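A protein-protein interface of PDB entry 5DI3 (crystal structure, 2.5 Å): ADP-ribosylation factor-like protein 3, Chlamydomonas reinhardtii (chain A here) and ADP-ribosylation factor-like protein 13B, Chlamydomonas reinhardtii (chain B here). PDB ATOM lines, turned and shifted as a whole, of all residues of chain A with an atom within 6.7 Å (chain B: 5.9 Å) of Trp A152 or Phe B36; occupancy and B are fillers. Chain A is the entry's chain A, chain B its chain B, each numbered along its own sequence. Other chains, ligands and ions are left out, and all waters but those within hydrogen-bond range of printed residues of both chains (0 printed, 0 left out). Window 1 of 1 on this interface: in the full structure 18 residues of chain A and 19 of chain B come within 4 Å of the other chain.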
ATOM      1  N   PRO A 119     -22.896  15.515   6.217  1.00  0.00           N
ATOM      2  CA  PRO A 119     -22.488  15.338   4.817  1.00  0.00           C
ATOM      3  C   PRO A 119     -23.659  15.498   3.846  1.00  0.00           C
ATOM      4  O   PRO A 119     -24.766  15.028   4.133  1.00  0.00           O
ATOM      5  CB  PRO A 119     -21.946  13.903   4.783  1.00  0.00           C
ATOM      6  CG  PRO A 119     -21.612  13.575   6.202  1.00  0.00           C
ATOM      7  CD  PRO A 119     -22.581  14.338   7.046  1.00  0.00           C
ATOM      8  N   LEU A 120     -23.416  16.163   2.719  1.00  0.00           N
ATOM      9  CA  LEU A 120     -24.467  16.412   1.736  1.00  0.00           C
ATOM     10  C   LEU A 120     -24.186  15.724   0.415  1.00  0.00           C
ATOM     11  O   LEU A 120     -23.185  15.993  -0.231  1.00  0.00           O
ATOM     12  CB  LEU A 120     -24.638  17.910   1.491  1.00  0.00           C
ATOM     13  CG  LEU A 120     -25.553  18.298   0.326  1.00  0.00           C
ATOM     14  CD1 LEU A 120     -26.974  17.790   0.543  1.00  0.00           C
ATOM     15  CD2 LEU A 120     -25.544  19.808   0.112  1.00  0.00           C
ATOM     16  N   LEU A 121     -25.079  14.835   0.013  1.00  0.00           N
ATOM     17  CA  LEU A 121     -25.024  14.264  -1.319  1.00  0.00           C
ATOM     18  C   LEU A 121     -26.176  14.823  -2.141  1.00  0.00           C
ATOM     19  O   LEU A 121     -27.346  14.675  -1.778  1.00  0.00           O
ATOM     20  CB  LEU A 121     -25.091  12.737  -1.261  1.00  0.00           C
ATOM     21  CG  LEU A 121     -25.248  11.998  -2.590  1.00  0.00           C
ATOM     22  CD1 LEU A 121     -23.966  12.096  -3.413  1.00  0.00           C
ATOM     23  CD2 LEU A 121     -25.625  10.546  -2.338  1.00  0.00           C
ATOM     24  N   VAL A 122     -25.841  15.485  -3.238  1.00  0.00           N
ATOM     25  CA  VAL A 122     -26.851  15.942  -4.176  1.00  0.00           C
ATOM     26  C   VAL A 122     -26.906  15.010  -5.374  1.00  0.00           C
ATOM     27  O   VAL A 122     -25.938  14.907  -6.119  1.00  0.00           O
ATOM     28  CB  VAL A 122     -26.577  17.368  -4.668  1.00  0.00           C
ATOM     29  CG1 VAL A 122     -27.553  17.731  -5.780  1.00  0.00           C
ATOM     30  CG2 VAL A 122     -26.666  18.356  -3.508  1.00  0.00           C
ATOM     31  N   ALA A 135     -23.128  18.780 -13.615  1.00  0.00           N
ATOM     32  CA  ALA A 135     -22.829  18.918 -12.192  1.00  0.00           C
ATOM     33  C   ALA A 135     -22.441  20.340 -11.794  1.00  0.00           C
ATOM     34  O   ALA A 135     -22.908  20.851 -10.776  1.00  0.00           O
ATOM     35  CB  ALA A 135     -21.719  17.952 -11.803  1.00  0.00           C
ATOM     36  N   ALA A 139     -24.350  22.998  -9.351  1.00  0.00           N
ATOM     37  CA  ALA A 139     -23.613  23.445  -8.175  1.00  0.00           C
ATOM     38  C   ALA A 139     -23.671  24.962  -8.007  1.00  0.00           C
ATOM     39  O   ALA A 139     -23.629  25.474  -6.885  1.00  0.00           O
ATOM     40  CB  ALA A 139     -22.169  22.980  -8.255  1.00  0.00           C
ATOM     41  N   ASP A 143     -26.224  27.300  -5.453  1.00  0.00           N
ATOM     42  CA  ASP A 143     -25.314  28.006  -4.551  1.00  0.00           C
ATOM     43  C   ASP A 143     -24.512  27.040  -3.661  1.00  0.00           C
ATOM     44  O   ASP A 143     -24.139  27.376  -2.535  1.00  0.00           O
ATOM     45  CB  ASP A 143     -26.103  29.006  -3.691  1.00  0.00           C
ATOM     46  CG  ASP A 143     -25.205  29.944  -2.895  1.00  0.00           C
ATOM     47  OD1 ASP A 143     -24.186  30.410  -3.449  1.00  0.00           O
ATOM     48  OD2 ASP A 143     -25.513  30.203  -1.710  1.00  0.00           O
ATOM     49  N   LEU A 144     -24.241  25.839  -4.167  1.00  0.00           N
ATOM     50  CA  LEU A 144     -23.436  24.871  -3.421  1.00  0.00           C
ATOM     51  C   LEU A 144     -22.007  25.383  -3.211  1.00  0.00           C
ATOM     52  O   LEU A 144     -21.380  25.110  -2.187  1.00  0.00           O
ATOM     53  CB  LEU A 144     -23.400  23.518  -4.138  1.00  0.00           C
ATOM     54  CG  LEU A 144     -24.724  22.801  -4.404  1.00  0.00           C
ATOM     55  CD1 LEU A 144     -24.477  21.479  -5.113  1.00  0.00           C
ATOM     56  CD2 LEU A 144     -25.496  22.578  -3.107  1.00  0.00           C
ATOM     57  N   THR A 145     -21.503  26.139  -4.181  1.00  0.00           N
ATOM     58  CA  THR A 145     -20.123  26.613  -4.146  1.00  0.00           C
ATOM     59  C   THR A 145     -19.873  27.685  -3.080  1.00  0.00           C
ATOM     60  O   THR A 145     -18.759  28.198  -2.957  1.00  0.00           O
ATOM     61  CB  THR A 145     -19.704  27.176  -5.510  1.00  0.00           C
ATOM     62  OG1 THR A 145     -20.531  28.298  -5.837  1.00  0.00           O
ATOM     63  CG2 THR A 145     -19.846  26.111  -6.595  1.00  0.00           C
ATOM     64  N   SER A 146     -20.903  28.024  -2.313  1.00  0.00           N
ATOM     65  CA  SER A 146     -20.744  28.973  -1.218  1.00  0.00           C
ATOM     66  C   SER A 146     -20.491  28.241   0.094  1.00  0.00           C
ATOM     67  O   SER A 146     -19.990  28.823   1.052  1.00  0.00           O
ATOM     68  CB  SER A 146     -21.973  29.871  -1.093  1.00  0.00           C
ATOM     69  OG  SER A 146     -21.978  30.864  -2.103  1.00  0.00           O
ATOM     70  N   ILE A 147     -20.823  26.955   0.117  1.00  0.00           N
ATOM     71  CA  ILE A 147     -20.698  26.146   1.323  1.00  0.00           C
ATOM     72  C   ILE A 147     -19.252  25.985   1.799  1.00  0.00           C
ATOM     73  O   ILE A 147     -18.355  25.721   0.999  1.00  0.00           O
ATOM     74  CB  ILE A 147     -21.297  24.751   1.106  1.00  0.00           C
ATOM     75  CG1 ILE A 147     -22.815  24.845   0.904  1.00  0.00           C
ATOM     76  CG2 ILE A 147     -20.982  23.850   2.284  1.00  0.00           C
ATOM     77  CD1 ILE A 147     -23.453  23.544   0.449  1.00  0.00           C
ATOM     78  N   ARG A 148     -19.035  26.149   3.105  1.00  0.00           N
ATOM     79  CA  ARG A 148     -17.728  25.892   3.708  1.00  0.00           C
ATOM     80  C   ARG A 148     -17.813  24.986   4.936  1.00  0.00           C
ATOM     81  O   ARG A 148     -16.802  24.431   5.366  1.00  0.00           O
ATOM     82  CB  ARG A 148     -17.043  27.203   4.105  1.00  0.00           C
ATOM     83  CG  ARG A 148     -16.779  28.165   2.956  1.00  0.00           C
ATOM     84  CD  ARG A 148     -15.752  27.619   1.970  1.00  0.00           C
ATOM     85  NE  ARG A 148     -15.487  28.575   0.897  1.00  0.00           N
ATOM     86  CZ  ARG A 148     -16.177  28.646  -0.236  1.00  0.00           C
ATOM     87  NH1 ARG A 148     -17.181  27.811  -0.462  1.00  0.00           N
ATOM     88  NH2 ARG A 148     -15.867  29.559  -1.146  1.00  0.00           N
ATOM     89  N   ARG A 150     -19.646  22.139   5.493  1.00  0.00           N
ATOM     90  CA  ARG A 150     -19.933  20.716   5.326  1.00  0.00           C
ATOM     91  C   ARG A 150     -19.285  20.164   4.060  1.00  0.00           C
ATOM     92  O   ARG A 150     -19.087  20.892   3.089  1.00  0.00           O
ATOM     93  CB  ARG A 150     -21.445  20.465   5.276  1.00  0.00           C
ATOM     94  CG  ARG A 150     -22.094  20.924   3.977  1.00  0.00           C
ATOM     95  CD  ARG A 150     -23.599  20.743   3.993  1.00  0.00           C
ATOM     96  NE  ARG A 150     -24.232  21.656   4.938  1.00  0.00           N
ATOM     97  CZ  ARG A 150     -24.746  21.283   6.104  1.00  0.00           C
ATOM     98  NH1 ARG A 150     -24.717  20.007   6.466  1.00  0.00           N
ATOM     99  NH2 ARG A 150     -25.300  22.188   6.902  1.00  0.00           N
ATOM    100  N   PRO A 151     -18.942  18.871   4.069  1.00  0.00           N
ATOM    101  CA  PRO A 151     -18.499  18.229   2.825  1.00  0.00           C
ATOM    102  C   PRO A 151     -19.694  17.891   1.942  1.00  0.00           C
ATOM    103  O   PRO A 151     -20.732  17.506   2.475  1.00  0.00           O
ATOM    104  CB  PRO A 151     -17.800  16.960   3.310  1.00  0.00           C
ATOM    105  CG  PRO A 151     -18.450  16.660   4.643  1.00  0.00           C
ATOM    106  CD  PRO A 151     -18.842  17.979   5.241  1.00  0.00           C
ATOM    107  N   TRP A 152     -19.567  18.032   0.626  1.00  0.00           N
ATOM    108  CA  TRP A 152     -20.666  17.660  -0.258  1.00  0.00           C
ATOM    109  C   TRP A 152     -20.218  17.152  -1.620  1.00  0.00           C
ATOM    110  O   TRP A 152     -19.217  17.617  -2.169  1.00  0.00           O
ATOM    111  CB  TRP A 152     -21.627  18.838  -0.449  1.00  0.00           C
ATOM    112  CG  TRP A 152     -21.010  20.089  -0.996  1.00  0.00           C
ATOM    113  CD1 TRP A 152     -20.508  21.136  -0.277  1.00  0.00           C
ATOM    114  CD2 TRP A 152     -20.854  20.445  -2.379  1.00  0.00           C
ATOM    115  NE1 TRP A 152     -20.043  22.115  -1.124  1.00  0.00           N
ATOM    116  CE2 TRP A 152     -20.241  21.714  -2.418  1.00  0.00           C
ATOM    117  CE3 TRP A 152     -21.171  19.810  -3.586  1.00  0.00           C
ATOM    118  CZ2 TRP A 152     -19.931  22.362  -3.617  1.00  0.00           C
ATOM    119  CZ3 TRP A 152     -20.866  20.458  -4.779  1.00  0.00           C
ATOM    120  CH2 TRP A 152     -20.252  21.720  -4.783  1.00  0.00           C
ATOM    121  N   GLN A 153     -20.971  16.188  -2.148  1.00  0.00           N
ATOM    122  CA  GLN A 153     -20.822  15.717  -3.524  1.00  0.00           C
ATOM    123  C   GLN A 153     -22.044  16.059  -4.339  1.00  0.00           C
ATOM    124  O   GLN A 153     -23.171  15.917  -3.862  1.00  0.00           O
ATOM    125  CB  GLN A 153     -20.644  14.201  -3.589  1.00  0.00           C
ATOM    126  CG  GLN A 153     -19.258  13.686  -3.406  1.00  0.00           C
ATOM    127  CD  GLN A 153     -18.401  13.830  -4.619  1.00  0.00           C
ATOM    128  OE1 GLN A 153     -17.688  14.819  -4.765  1.00  0.00           O
ATOM    129  NE2 GLN A 153     -18.452  12.841  -5.502  1.00  0.00           N
ATOM    130  N   ILE A 154     -21.844  16.477  -5.579  1.00  0.00           N
ATOM    131  CA  ILE A 154     -22.951  16.392  -6.503  1.00  0.00           C
ATOM    132  C   ILE A 154     -22.672  15.247  -7.460  1.00  0.00           C
ATOM    133  O   ILE A 154     -21.645  15.203  -8.139  1.00  0.00           O
ATOM    134  CB  ILE A 154     -23.222  17.699  -7.257  1.00  0.00           C
ATOM    135  CG1 ILE A 154     -24.432  17.482  -8.165  1.00  0.00           C
ATOM    136  CG2 ILE A 154     -21.999  18.176  -8.026  1.00  0.00           C
ATOM    137  CD1 ILE A 154     -25.028  18.726  -8.674  1.00  0.00           C
ATOM    138  N   GLN A 155     -23.581  14.284  -7.458  1.00  0.00           N
ATOM    139  CA  GLN A 155     -23.416  13.093  -8.259  1.00  0.00           C
ATOM    140  C   GLN A 155     -24.489  13.051  -9.329  1.00  0.00           C
ATOM    141  O   GLN A 155     -25.656  12.765  -9.043  1.00  0.00           O
ATOM    142  CB  GLN A 155     -23.480  11.839  -7.391  1.00  0.00           C
ATOM    143  CG  GLN A 155     -23.487  10.550  -8.194  1.00  0.00           C
ATOM    144  CD  GLN A 155     -22.152  10.295  -8.878  1.00  0.00           C
ATOM    145  OE1 GLN A 155     -21.099  10.346  -8.244  1.00  0.00           O
ATOM    146  NE2 GLN A 155     -22.192  10.037 -10.180  1.00  0.00           N
ATOM    147  N   ALA A 156     -24.090  13.372 -10.556  1.00  0.00           N
ATOM    148  CA  ALA A 156     -24.970  13.236 -11.704  1.00  0.00           C
ATOM    149  C   ALA A 156     -25.442  11.795 -11.771  1.00  0.00           C
ATOM    150  O   ALA A 156     -24.665  10.865 -11.549  1.00  0.00           O
ATOM    151  CB  ALA A 156     -24.253  13.640 -12.995  1.00  0.00           C
ATOM    152  N   TRP A 171     -19.659   7.350  -2.014  1.00  0.00           N
ATOM    153  CA  TRP A 171     -19.126   8.534  -1.348  1.00  0.00           C
ATOM    154  C   TRP A 171     -19.778   8.734   0.009  1.00  0.00           C
ATOM    155  O   TRP A 171     -19.109   9.053   0.994  1.00  0.00           O
ATOM    156  CB  TRP A 171     -19.345   9.785  -2.195  1.00  0.00           C
ATOM    157  CG  TRP A 171     -18.894  11.044  -1.505  1.00  0.00           C
ATOM    158  CD1 TRP A 171     -17.633  11.577  -1.516  1.00  0.00           C
ATOM    159  CD2 TRP A 171     -19.692  11.924  -0.699  1.00  0.00           C
ATOM    160  NE1 TRP A 171     -17.604  12.736  -0.774  1.00  0.00           N
ATOM    161  CE2 TRP A 171     -18.857  12.970  -0.262  1.00  0.00           C
ATOM    162  CE3 TRP A 171     -21.038  11.933  -0.312  1.00  0.00           C
ATOM    163  CZ2 TRP A 171     -19.316  14.013   0.541  1.00  0.00           C
ATOM    164  CZ3 TRP A 171     -21.492  12.968   0.488  1.00  0.00           C
ATOM    165  CH2 TRP A 171     -20.634  13.991   0.907  1.00  0.00           C
ATOM    166  N   PRO B  34     -13.724   9.448  -7.319  1.00  0.00           N
ATOM    167  CA  PRO B  34     -13.654  10.795  -7.904  1.00  0.00           C
ATOM    168  C   PRO B  34     -14.329  11.854  -7.027  1.00  0.00           C
ATOM    169  O   PRO B  34     -15.300  11.544  -6.329  1.00  0.00           O
ATOM    170  CB  PRO B  34     -14.400  10.637  -9.234  1.00  0.00           C
ATOM    171  CG  PRO B  34     -14.200   9.194  -9.601  1.00  0.00           C
ATOM    172  CD  PRO B  34     -14.200   8.442  -8.290  1.00  0.00           C
ATOM    173  N   THR B  35     -13.814  13.080  -7.051  1.00  0.00           N
ATOM    174  CA  THR B  35     -14.402  14.171  -6.281  1.00  0.00           C
ATOM    175  C   THR B  35     -15.253  15.064  -7.177  1.00  0.00           C
ATOM    176  O   THR B  35     -14.791  15.532  -8.220  1.00  0.00           O
ATOM    177  CB  THR B  35     -13.321  15.038  -5.584  1.00  0.00           C
ATOM    178  OG1 THR B  35     -12.478  14.202  -4.780  1.00  0.00           O
ATOM    179  CG2 THR B  35     -13.969  16.103  -4.703  1.00  0.00           C
ATOM    180  N   PHE B  36     -16.499  15.286  -6.772  1.00  0.00           N
ATOM    181  CA  PHE B  36     -17.391  16.193  -7.489  1.00  0.00           C
ATOM    182  C   PHE B  36     -18.033  17.164  -6.511  1.00  0.00           C
ATOM    183  O   PHE B  36     -19.248  17.168  -6.333  1.00  0.00           O
ATOM    184  CB  PHE B  36     -18.464  15.417  -8.254  1.00  0.00           C
ATOM    185  CG  PHE B  36     -17.977  14.827  -9.546  1.00  0.00           C
ATOM    186  CD1 PHE B  36     -17.425  13.554  -9.581  1.00  0.00           C
ATOM    187  CD2 PHE B  36     -18.066  15.548 -10.727  1.00  0.00           C
ATOM    188  CE1 PHE B  36     -16.974  13.008 -10.776  1.00  0.00           C
ATOM    189  CE2 PHE B  36     -17.618  15.012 -11.925  1.00  0.00           C
ATOM    190  CZ  PHE B  36     -17.070  13.740 -11.949  1.00  0.00           C
ATOM    191  N   GLY B  37     -17.205  17.985  -5.873  1.00  0.00           N
ATOM    192  CA  GLY B  37     -17.701  18.927  -4.892  1.00  0.00           C
ATOM    193  C   GLY B  37     -16.614  19.564  -4.054  1.00  0.00           C
ATOM    194  O   GLY B  37     -15.553  19.934  -4.561  1.00  0.00           O
ATOM    195  N   PHE B  38     -16.885  19.682  -2.760  1.00  0.00           N
ATOM    196  CA  PHE B  38     -16.022  20.422  -1.852  1.00  0.00           C
ATOM    197  C   PHE B  38     -15.712  19.588  -0.612  1.00  0.00           C
ATOM    198  O   PHE B  38     -16.532  18.779  -0.176  1.00  0.00           O
ATOM    199  CB  PHE B  38     -16.687  21.753  -1.481  1.00  0.00           C
ATOM    200  CG  PHE B  38     -16.068  22.447  -0.298  1.00  0.00           C
ATOM    201  CD1 PHE B  38     -14.987  23.298  -0.465  1.00  0.00           C
ATOM    202  CD2 PHE B  38     -16.588  22.272   0.975  1.00  0.00           C
ATOM    203  CE1 PHE B  38     -14.419  23.946   0.619  1.00  0.00           C
ATOM    204  CE2 PHE B  38     -16.027  22.918   2.064  1.00  0.00           C
ATOM    205  CZ  PHE B  38     -14.938  23.756   1.885  1.00  0.00           C
ATOM    206  N   ASN B  39     -14.521  19.786  -0.056  1.00  0.00           N
ATOM    207  CA  ASN B  39     -14.087  19.039   1.119  1.00  0.00           C
ATOM    208  C   ASN B  39     -12.939  19.756   1.833  1.00  0.00           C
ATOM    209  O   ASN B  39     -11.826  19.837   1.315  1.00  0.00           O
ATOM    210  CB  ASN B  39     -13.671  17.623   0.715  1.00  0.00           C
ATOM    211  CG  ASN B  39     -13.670  16.661   1.880  1.00  0.00           C
ATOM    212  OD1 ASN B  39     -12.787  16.707   2.735  1.00  0.00           O
ATOM    213  ND2 ASN B  39     -14.662  15.774   1.921  1.00  0.00           N
ATOM    214  N   GLY B  56     -12.755  18.712  -7.102  1.00  0.00           N
ATOM    215  CA  GLY B  56     -12.701  17.823  -8.247  1.00  0.00           C
ATOM    216  C   GLY B  56     -12.100  18.514  -9.452  1.00  0.00           C
ATOM    217  O   GLY B  56     -12.170  19.741  -9.585  1.00  0.00           O
ATOM    218  N   GLY B  58     -12.534  16.976 -12.706  1.00  0.00           N
ATOM    219  CA  GLY B  58     -13.200  16.450 -13.882  1.00  0.00           C
ATOM    220  C   GLY B  58     -13.758  17.585 -14.716  1.00  0.00           C
ATOM    221  O   GLY B  58     -14.052  18.660 -14.186  1.00  0.00           O
ATOM    222  N   ASN B  60     -16.579  18.190 -15.888  1.00  0.00           N
ATOM    223  CA  ASN B  60     -17.911  18.647 -15.530  1.00  0.00           C
ATOM    224  C   ASN B  60     -17.995  19.294 -14.154  1.00  0.00           C
ATOM    225  O   ASN B  60     -19.086  19.614 -13.688  1.00  0.00           O
ATOM    226  CB  ASN B  60     -18.893  17.479 -15.601  1.00  0.00           C
ATOM    227  CG  ASN B  60     -19.196  17.063 -17.025  1.00  0.00           C
ATOM    228  OD1 ASN B  60     -19.324  17.909 -17.912  1.00  0.00           O
ATOM    229  ND2 ASN B  60     -19.309  15.754 -17.254  1.00  0.00           N
ATOM    230  N   ILE B  61     -16.854  19.481 -13.499  1.00  0.00           N
ATOM    231  CA  ILE B  61     -16.857  20.116 -12.186  1.00  0.00           C
ATOM    232  C   ILE B  61     -15.729  21.133 -12.035  1.00  0.00           C
ATOM    233  O   ILE B  61     -15.808  22.011 -11.189  1.00  0.00           O
ATOM    234  CB  ILE B  61     -16.762  19.064 -11.038  1.00  0.00           C
ATOM    235  CG1 ILE B  61     -17.267  19.648  -9.714  1.00  0.00           C
ATOM    236  CG2 ILE B  61     -15.349  18.518 -10.894  1.00  0.00           C
ATOM    237  CD1 ILE B  61     -18.552  20.432  -9.839  1.00  0.00           C
ATOM    238  N   VAL B  64     -15.772  24.956 -11.446  1.00  0.00           N
ATOM    239  CA  VAL B  64     -16.168  25.452 -10.138  1.00  0.00           C
ATOM    240  C   VAL B  64     -14.980  26.113  -9.408  1.00  0.00           C
ATOM    241  O   VAL B  64     -15.181  26.984  -8.556  1.00  0.00           O
ATOM    242  CB  VAL B  64     -16.786  24.296  -9.304  1.00  0.00           C
ATOM    243  CG1 VAL B  64     -16.752  24.573  -7.834  1.00  0.00           C
ATOM    244  CG2 VAL B  64     -18.222  24.040  -9.750  1.00  0.00           C
ATOM    245  N   TYR B  68     -13.583  29.768  -5.874  1.00  0.00           N
ATOM    246  CA  TYR B  68     -12.845  29.696  -4.615  1.00  0.00           C
ATOM    247  C   TYR B  68     -11.571  30.534  -4.586  1.00  0.00           C
ATOM    248  O   TYR B  68     -11.064  30.840  -3.508  1.00  0.00           O
ATOM    249  CB  TYR B  68     -12.473  28.244  -4.296  1.00  0.00           C
ATOM    250  CG  TYR B  68     -13.653  27.315  -4.146  1.00  0.00           C
ATOM    251  CD1 TYR B  68     -14.215  27.064  -2.903  1.00  0.00           C
ATOM    252  CD2 TYR B  68     -14.202  26.685  -5.249  1.00  0.00           C
ATOM    253  CE1 TYR B  68     -15.295  26.211  -2.769  1.00  0.00           C
ATOM    254  CE2 TYR B  68     -15.271  25.836  -5.124  1.00  0.00           C
ATOM    255  CZ  TYR B  68     -15.817  25.600  -3.889  1.00  0.00           C
ATOM    256  OH  TYR B  68     -16.889  24.747  -3.789  1.00  0.00           O
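Asn B60 touches Ala A135. Thr A145 touches Val B64 (CG2 to CG1, 3.7 Å). Ile A147 touches Phe B38 (O to CE2, 3.8 Å). Phe B38 touches Arg A148. Arg A148 touches Tyr B68 (NH1 to CE1, 3.4 Å). ND2 of Asn B39 touches CB of Pro A151, at 3.6 Å. CZ3 of Trp A152 touches O of Phe B36, 3.98 Å away. Gly B37 touches Trp A152 (CA to O, 3.4 Å). Tyr B68 touches Trp A152. Gln A153 touches Thr B35.
O of Phe B36 is in hydrogen-bond range of N of Ile A154 (2.8 Å). The backbone NH (N) of Phe B38 lies within hydrogen-bond range of the backbone carbonyl oxygen (O) of Trp A152, 3.2 Å away. N of Gly B37 is in hydrogen-bond range of OE1 of Gln A153. OE1 of Gln A153 lies close to O of Phe B36 (3.2 Å).
Leu A120 touches none of the printed residues of chain B. Leu A121 touches none of the printed residues of chain B. Of the printed residues of chain B, Ala A135 touches Asn B60 (3.6 Å). Of the printed residues of chain B, Trp A152 touches Phe B36 (3.98 Å), Gly B37 (3.4 Å), Phe B38 (3.2 Å) and Tyr B68 (3.9 Å). Of the printed residues of chain A, Pro B34 touches Gln A153 (3.5 Å). Of the printed residues of chain A, Phe B36 touches Trp A152, Gln A153 and Ile A154. Of the printed residues of chain A, Asn B39 touches Pro A151 (3.6 Å). Of the printed residues of chain A, Asn B60 touches Ala A135 (3.6 Å).
Printed residues of chain B that touch a printed residue of chain A: Pro B34, Thr B35, Phe B36, Gly B37, Phe B38, Asn B39, Asn B60, Val B64 and Tyr B68. Hydrophobic or aromatic side chains of chain B that line the printed part of chain A: Phe B36, Phe B38, Val B64 and Tyr B68. Of the 20 printed residues of chain A, 9 touch a printed residue of chain B. Among the printed residues, 18 pairs touch across the chains.
The indole nitrogen (NE1) of Trp A152 lies close to the backbone carbonyl oxygen (O) of Leu A144, 3.4 Å away. The backbone NH of Gln A153 lies within hydrogen-bond range of the backbone carbonyl oxygen of Leu A120, 2.9 Å away. The backbone NH of Leu A120 is in hydrogen-bond range of the backbone carbonyl oxygen of Pro A151 (3.0 Å). The backbone carbonyl oxygen (O) of Ser A146 is in hydrogen-bond range of the guanidinium group (NH1) of Arg A148 (3.3 Å). O of Thr A145 sits at hydrogen-bond distance from NH1 of Arg A148 (3.0 Å). The backbone carbonyl oxygen of Gln A153 is in hydrogen-bond range of the backbone NH of Val A122, 2.8 Å away.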
